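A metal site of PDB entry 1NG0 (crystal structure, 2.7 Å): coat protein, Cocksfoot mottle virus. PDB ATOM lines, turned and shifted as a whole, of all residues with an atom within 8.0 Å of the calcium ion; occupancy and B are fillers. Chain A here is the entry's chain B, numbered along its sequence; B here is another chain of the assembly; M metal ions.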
ATOM      1  N   ALA A 102      22.374  -7.371  28.403  1.00  0.00           N
ATOM      2  CA  ALA A 102      23.280  -8.461  28.748  1.00  0.00           C
ATOM      3  C   ALA A 102      23.266  -9.605  27.757  1.00  0.00           C
ATOM      4  O   ALA A 102      24.268 -10.295  27.586  1.00  0.00           O
ATOM      5  CB  ALA A 102      22.935  -8.994  30.126  1.00  0.00           C
ATOM      6  N   LYS A 103      22.142  -9.801  27.082  1.00  0.00           N
ATOM      7  CA  LYS A 103      22.065 -10.918  26.156  1.00  0.00           C
ATOM      8  C   LYS A 103      23.076 -10.874  25.029  1.00  0.00           C
ATOM      9  O   LYS A 103      23.427 -11.905  24.471  1.00  0.00           O
ATOM     10  CB  LYS A 103      20.645 -11.062  25.613  1.00  0.00           C
ATOM     11  CG  LYS A 103      20.318 -12.516  25.364  1.00  0.00           C
ATOM     12  CD  LYS A 103      18.868 -12.830  25.606  1.00  0.00           C
ATOM     13  CE  LYS A 103      18.668 -14.320  25.936  1.00  0.00           C
ATOM     14  NZ  LYS A 103      19.252 -15.248  24.914  1.00  0.00           N
ATOM     15  N   TYR A 105      26.149 -10.185  25.377  1.00  0.00           N
ATOM     16  CA  TYR A 105      27.474 -10.415  25.945  1.00  0.00           C
ATOM     17  C   TYR A 105      27.595 -11.791  26.576  1.00  0.00           C
ATOM     18  O   TYR A 105      26.595 -12.361  27.012  1.00  0.00           O
ATOM     19  CB  TYR A 105      27.794  -9.354  26.991  1.00  0.00           C
ATOM     20  CG  TYR A 105      27.900  -7.968  26.408  1.00  0.00           C
ATOM     21  CD1 TYR A 105      26.779  -7.130  26.297  1.00  0.00           C
ATOM     22  CD2 TYR A 105      29.120  -7.500  25.946  1.00  0.00           C
ATOM     23  CE1 TYR A 105      26.886  -5.861  25.730  1.00  0.00           C
ATOM     24  CE2 TYR A 105      29.234  -6.237  25.378  1.00  0.00           C
ATOM     25  CZ  TYR A 105      28.121  -5.421  25.274  1.00  0.00           C
ATOM     26  OH  TYR A 105      28.277  -4.185  24.692  1.00  0.00           O
ATOM     27  N   ALA A 106      28.811 -12.323  26.644  1.00  0.00           N
ATOM     28  CA  ALA A 106      29.016 -13.646  27.200  1.00  0.00           C
ATOM     29  C   ALA A 106      29.352 -13.679  28.673  1.00  0.00           C
ATOM     30  O   ALA A 106      28.975 -14.626  29.375  1.00  0.00           O
ATOM     31  CB  ALA A 106      30.103 -14.352  26.431  1.00  0.00           C
ATOM     32  N   LEU A 107      30.062 -12.657  29.155  1.00  0.00           N
ATOM     33  CA  LEU A 107      30.482 -12.595  30.558  1.00  0.00           C
ATOM     34  C   LEU A 107      29.954 -11.378  31.273  1.00  0.00           C
ATOM     35  O   LEU A 107      29.604 -10.384  30.657  1.00  0.00           O
ATOM     36  CB  LEU A 107      32.003 -12.555  30.633  1.00  0.00           C
ATOM     37  CG  LEU A 107      32.743 -13.476  29.681  1.00  0.00           C
ATOM     38  CD1 LEU A 107      34.234 -13.238  29.761  1.00  0.00           C
ATOM     39  CD2 LEU A 107      32.416 -14.900  30.040  1.00  0.00           C
ATOM     40  N   PHE A 194      31.652 -14.012  35.384  1.00  0.00           N
ATOM     41  CA  PHE A 194      30.666 -15.079  35.353  1.00  0.00           C
ATOM     42  C   PHE A 194      30.112 -15.206  33.944  1.00  0.00           C
ATOM     43  O   PHE A 194      30.079 -14.229  33.200  1.00  0.00           O
ATOM     44  CB  PHE A 194      29.514 -14.782  36.304  1.00  0.00           C
ATOM     45  CG  PHE A 194      29.900 -14.831  37.744  1.00  0.00           C
ATOM     46  CD1 PHE A 194      30.441 -13.714  38.361  1.00  0.00           C
ATOM     47  CD2 PHE A 194      29.717 -15.989  38.487  1.00  0.00           C
ATOM     48  CE1 PHE A 194      30.790 -13.746  39.713  1.00  0.00           C
ATOM     49  CE2 PHE A 194      30.059 -16.028  39.839  1.00  0.00           C
ATOM     50  CZ  PHE A 194      30.599 -14.909  40.446  1.00  0.00           C
ATOM     51  N   LYS A 195      29.696 -16.418  33.575  1.00  0.00           N
ATOM     52  CA  LYS A 195      29.130 -16.627  32.256  1.00  0.00           C
ATOM     53  C   LYS A 195      27.637 -16.347  32.362  1.00  0.00           C
ATOM     54  O   LYS A 195      26.953 -16.910  33.218  1.00  0.00           O
ATOM     55  CB  LYS A 195      29.352 -18.063  31.790  1.00  0.00           C
ATOM     56  CG  LYS A 195      30.767 -18.580  31.978  1.00  0.00           C
ATOM     57  CD  LYS A 195      31.760 -17.742  31.223  1.00  0.00           C
ATOM     58  CE  LYS A 195      33.190 -18.187  31.521  1.00  0.00           C
ATOM     59  NZ  LYS A 195      33.508 -19.522  30.935  1.00  0.00           N
ATOM     60  N   LEU A 196      27.122 -15.474  31.501  1.00  0.00           N
ATOM     61  CA  LEU A 196      25.704 -15.147  31.522  1.00  0.00           C
ATOM     62  C   LEU A 196      24.843 -16.356  31.159  1.00  0.00           C
ATOM     63  O   LEU A 196      25.013 -16.968  30.092  1.00  0.00           O
ATOM     64  CB  LEU A 196      25.433 -13.996  30.571  1.00  0.00           C
ATOM     65  CG  LEU A 196      25.942 -12.654  31.096  1.00  0.00           C
ATOM     66  CD1 LEU A 196      26.073 -11.641  29.972  1.00  0.00           C
ATOM     67  CD2 LEU A 196      24.981 -12.163  32.169  1.00  0.00           C
ATOM     68  N   SER A 197      23.916 -16.697  32.046  1.00  0.00           N
ATOM     69  CA  SER A 197      23.028 -17.839  31.824  1.00  0.00           C
ATOM     70  C   SER A 197      21.567 -17.426  31.835  1.00  0.00           C
ATOM     71  O   SER A 197      21.138 -16.661  32.693  1.00  0.00           O
ATOM     72  CB  SER A 197      23.257 -18.905  32.896  1.00  0.00           C
ATOM     73  OG  SER A 197      22.424 -20.031  32.665  1.00  0.00           O
ATOM     74  N   TRP A 198      20.797 -17.954  30.882  1.00  0.00           N
ATOM     75  CA  TRP A 198      19.392 -17.628  30.801  1.00  0.00           C
ATOM     76  C   TRP A 198      18.425 -18.746  31.178  1.00  0.00           C
ATOM     77  O   TRP A 198      17.213 -18.603  31.031  1.00  0.00           O
ATOM     78  CB  TRP A 198      19.058 -17.114  29.409  1.00  0.00           C
ATOM     79  CG  TRP A 198      19.120 -15.646  29.361  1.00  0.00           C
ATOM     80  CD1 TRP A 198      18.103 -14.768  29.617  1.00  0.00           C
ATOM     81  CD2 TRP A 198      20.290 -14.847  29.153  1.00  0.00           C
ATOM     82  NE1 TRP A 198      18.570 -13.465  29.603  1.00  0.00           N
ATOM     83  CE2 TRP A 198      19.910 -13.488  29.320  1.00  0.00           C
ATOM     84  CE3 TRP A 198      21.619 -15.155  28.865  1.00  0.00           C
ATOM     85  CZ2 TRP A 198      20.817 -12.451  29.186  1.00  0.00           C
ATOM     86  CZ3 TRP A 198      22.526 -14.118  28.731  1.00  0.00           C
ATOM     87  CH2 TRP A 198      22.118 -12.774  28.896  1.00  0.00           C
ATOM     88  N   VAL A 247      28.772 -12.256  21.754  1.00  0.00           N
ATOM     89  CA  VAL A 247      27.980 -13.434  21.374  1.00  0.00           C
ATOM     90  C   VAL A 247      26.667 -13.013  20.770  1.00  0.00           C
ATOM     91  O   VAL A 247      26.192 -11.908  21.016  1.00  0.00           O
ATOM     92  CB  VAL A 247      27.580 -14.355  22.544  1.00  0.00           C
ATOM     93  CG1 VAL A 247      28.768 -15.142  22.993  1.00  0.00           C
ATOM     94  CG2 VAL A 247      26.998 -13.539  23.663  1.00  0.00           C
ATOM     95  N   SER A 248      26.066 -13.897  19.991  1.00  0.00           N
ATOM     96  CA  SER A 248      24.789 -13.596  19.381  1.00  0.00           C
ATOM     97  C   SER A 248      23.730 -13.839  20.444  1.00  0.00           C
ATOM     98  O   SER A 248      23.699 -14.895  21.067  1.00  0.00           O
ATOM     99  CB  SER A 248      24.530 -14.519  18.200  1.00  0.00           C
ATOM    100  OG  SER A 248      23.220 -14.283  17.704  1.00  0.00           O
ATOM    101  N   PRO A 249      22.845 -12.862  20.659  1.00  0.00           N
ATOM    102  CA  PRO A 249      21.791 -13.020  21.662  1.00  0.00           C
ATOM    103  C   PRO A 249      21.061 -14.360  21.554  1.00  0.00           C
ATOM    104  O   PRO A 249      20.812 -15.030  22.561  1.00  0.00           O
ATOM    105  CB  PRO A 249      20.863 -11.844  21.369  1.00  0.00           C
ATOM    106  CG  PRO A 249      21.808 -10.804  20.882  1.00  0.00           C
ATOM    107  CD  PRO A 249      22.696 -11.577  19.946  1.00  0.00           C
ATOM    108  N   THR A 251      22.140 -17.214  20.524  1.00  0.00           N
ATOM    109  CA  THR A 251      22.927 -18.399  20.879  1.00  0.00           C
ATOM    110  C   THR A 251      23.383 -18.321  22.334  1.00  0.00           C
ATOM    111  O   THR A 251      24.049 -19.233  22.825  1.00  0.00           O
ATOM    112  CB  THR A 251      24.170 -18.553  19.985  1.00  0.00           C
ATOM    113  OG1 THR A 251      25.125 -17.544  20.301  1.00  0.00           O
ATOM    114  CG2 THR A 251      23.782 -18.415  18.526  1.00  0.00           C
ATOM    115  N   ASN A 252      23.005 -17.248  23.008  1.00  0.00           N
ATOM    116  CA  ASN A 252      23.395 -17.042  24.400  1.00  0.00           C
ATOM    117  C   ASN A 252      22.438 -17.755  25.351  1.00  0.00           C
ATOM    118  O   ASN A 252      21.290 -17.329  25.511  1.00  0.00           O
ATOM    119  CB  ASN A 252      23.404 -15.551  24.728  1.00  0.00           C
ATOM    120  CG  ASN A 252      24.138 -15.237  26.018  1.00  0.00           C
ATOM    121  OD1 ASN A 252      24.299 -16.101  26.895  1.00  0.00           O
ATOM    122  ND2 ASN A 252      24.580 -13.996  26.158  1.00  0.00           N
ATOM    123  N   LEU A 253      22.923 -18.813  25.977  1.00  0.00           N
ATOM    124  CA  LEU A 253      22.094 -19.580  26.910  1.00  0.00           C
ATOM    125  C   LEU A 253      22.727 -19.615  28.308  1.00  0.00           C
ATOM    126  O   LEU A 253      23.898 -19.152  28.451  1.00  0.00           O
ATOM    127  CB  LEU A 253      21.940 -21.004  26.380  1.00  0.00           C
ATOM    128  CG  LEU A 253      21.612 -21.090  24.892  1.00  0.00           C
ATOM    129  CD1 LEU A 253      21.685 -22.521  24.429  1.00  0.00           C
ATOM    130  CD2 LEU A 253      20.237 -20.508  24.641  1.00  0.00           C
ATOM    131  OXT LEU A 253      22.051 -20.109  29.243  1.00  0.00           O
ATOM    132  N   LEU B 135      32.828 -18.182  24.501  1.00  0.00           N
ATOM    133  CA  LEU B 135      33.339 -18.079  25.867  1.00  0.00           C
ATOM    134  C   LEU B 135      32.553 -18.807  26.946  1.00  0.00           C
ATOM    135  O   LEU B 135      33.014 -18.898  28.097  1.00  0.00           O
ATOM    136  CB  LEU B 135      33.483 -16.614  26.241  1.00  0.00           C
ATOM    137  CG  LEU B 135      34.233 -15.783  25.187  1.00  0.00           C
ATOM    138  CD1 LEU B 135      34.251 -14.324  25.602  1.00  0.00           C
ATOM    139  CD2 LEU B 135      35.643 -16.312  25.020  1.00  0.00           C
ATOM    140  N   ASP B 136      31.359 -19.295  26.608  1.00  0.00           N
ATOM    141  CA  ASP B 136      30.516 -20.021  27.556  1.00  0.00           C
ATOM    142  C   ASP B 136      30.211 -21.385  26.935  1.00  0.00           C
ATOM    143  O   ASP B 136      29.626 -21.462  25.865  1.00  0.00           O
ATOM    144  CB  ASP B 136      29.209 -19.252  27.812  1.00  0.00           C
ATOM    145  CG  ASP B 136      28.260 -19.986  28.761  1.00  0.00           C
ATOM    146  OD1 ASP B 136      28.659 -21.061  29.285  1.00  0.00           O
ATOM    147  OD2 ASP B 136      27.119 -19.503  28.978  1.00  0.00           O
ATOM    148  N   TYR B 137      30.612 -22.449  27.602  1.00  0.00           N
ATOM    149  CA  TYR B 137      30.386 -23.788  27.074  1.00  0.00           C
ATOM    150  C   TYR B 137      28.909 -24.079  26.845  1.00  0.00           C
ATOM    151  O   TYR B 137      28.561 -24.944  26.046  1.00  0.00           O
ATOM    152  CB  TYR B 137      30.968 -24.848  28.001  1.00  0.00           C
ATOM    153  CG  TYR B 137      31.494 -26.044  27.238  1.00  0.00           C
ATOM    154  CD1 TYR B 137      32.731 -25.997  26.612  1.00  0.00           C
ATOM    155  CD2 TYR B 137      30.734 -27.198  27.123  1.00  0.00           C
ATOM    156  CE1 TYR B 137      33.200 -27.069  25.876  1.00  0.00           C
ATOM    157  CE2 TYR B 137      31.196 -28.290  26.375  1.00  0.00           C
ATOM    158  CZ  TYR B 137      32.439 -28.209  25.763  1.00  0.00           C
ATOM    159  OH  TYR B 137      32.901 -29.272  25.008  1.00  0.00           O
ATOM    160  N   ALA B 138      28.040 -23.371  27.551  1.00  0.00           N
ATOM    161  CA  ALA B 138      26.605 -23.574  27.424  1.00  0.00           C
ATOM    162  C   ALA B 138      26.003 -22.869  26.201  1.00  0.00           C
ATOM    163  O   ALA B 138      24.912 -23.208  25.760  1.00  0.00           O
ATOM    164  CB  ALA B 138      25.901 -23.105  28.682  1.00  0.00           C
ATOM    165  N   ASP B 139      26.700 -21.863  25.673  1.00  0.00           N
ATOM    166  CA  ASP B 139      26.183 -21.151  24.510  1.00  0.00           C
ATOM    167  C   ASP B 139      26.165 -22.131  23.348  1.00  0.00           C
ATOM    168  O   ASP B 139      27.008 -23.026  23.274  1.00  0.00           O
ATOM    169  CB  ASP B 139      27.057 -19.932  24.177  1.00  0.00           C
ATOM    170  CG  ASP B 139      26.981 -18.834  25.244  1.00  0.00           C
ATOM    171  OD1 ASP B 139      25.935 -18.723  25.927  1.00  0.00           O
ATOM    172  OD2 ASP B 139      27.965 -18.073  25.377  1.00  0.00           O
ATOM    173  N   SER B 140      25.212 -21.975  22.443  1.00  0.00           N
ATOM    174  CA  SER B 140      25.122 -22.872  21.293  1.00  0.00           C
ATOM    175  C   SER B 140      26.030 -22.415  20.169  1.00  0.00           C
ATOM    176  O   SER B 140      26.391 -21.238  20.071  1.00  0.00           O
ATOM    177  CB  SER B 140      23.681 -22.958  20.798  1.00  0.00           C
ATOM    178  OG  SER B 140      23.217 -21.689  20.370  1.00  0.00           O
ATOM    179  N   HIS B 208      27.685 -26.581  32.131  1.00  0.00           N
ATOM    180  CA  HIS B 208      28.197 -25.678  33.145  1.00  0.00           C
ATOM    181  C   HIS B 208      29.469 -26.243  33.762  1.00  0.00           C
ATOM    182  O   HIS B 208      30.419 -25.504  34.014  1.00  0.00           O
ATOM    183  CB  HIS B 208      27.161 -25.454  34.236  1.00  0.00           C
ATOM    184  CG  HIS B 208      25.966 -24.687  33.774  1.00  0.00           C
ATOM    185  ND1 HIS B 208      26.072 -23.512  33.054  1.00  0.00           N
ATOM    186  CD2 HIS B 208      24.641 -24.904  33.936  1.00  0.00           C
ATOM    187  CE1 HIS B 208      24.855 -23.041  32.797  1.00  0.00           C
ATOM    188  NE2 HIS B 208      23.979 -23.870  33.319  1.00  0.00           N
ATOM    189  N   ASP B 211      32.401 -26.070  31.406  1.00  0.00           N
ATOM    190  CA  ASP B 211      32.810 -24.685  31.302  1.00  0.00           C
ATOM    191  C   ASP B 211      33.865 -24.290  32.316  1.00  0.00           C
ATOM    192  O   ASP B 211      34.694 -23.415  32.051  1.00  0.00           O
ATOM    193  CB  ASP B 211      31.586 -23.775  31.464  1.00  0.00           C
ATOM    194  CG  ASP B 211      31.914 -22.333  31.187  1.00  0.00           C
ATOM    195  OD1 ASP B 211      32.243 -22.007  30.035  1.00  0.00           O
ATOM    196  OD2 ASP B 211      31.839 -21.520  32.137  1.00  0.00           O
HETATM  197 CA    CA M   1      25.809 -17.760  28.006  1.00  0.00          CA
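The calcium ion is bound by the side-chain carboxylate (OD1) of Asp 139 of chain B (2.3 Å), the backbone carbonyl oxygen (O) of Leu 196 (2.4 Å), the side-chain carboxylate (OD2) of Asp 136 of chain B (2.4 Å), the chain-end carboxylate (O) of Leu 253 (2.4 Å) and the side-chain amide oxygen (OD1) of Asn 252 (2.5 Å).
The calcium ion has five donor atoms within binding distance.
N of Trp 198 lies within hydrogen-bond range of OXT of Leu 253.
O of Tyr 105 is in hydrogen-bond range of ND2 of Asn 252 (2.7 Å).
ND2 of Asn 252 sits at hydrogen-bond distance from O of Lys 103 (2.9 Å).
The side-chain hydroxyl (OG) of Ser 197 lies within hydrogen-bond range of the chain-end carboxylate (OXT) of Leu 253 (3.4 Å).
N of Leu 196 lies within hydrogen-bond range of O of Ala 106 (2.9 Å).
The side-chain carboxylate (OD1) of Asp 136 of chain B is in hydrogen-bond range of the backbone NH (N) of Ala 138 of chain B (3.0 Å).
Five residues have an atom within 4 Å of the calcium ion: Leu 196, Asn 252, Leu 253, Asp 136 of chain B and Asp 139 of chain B.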
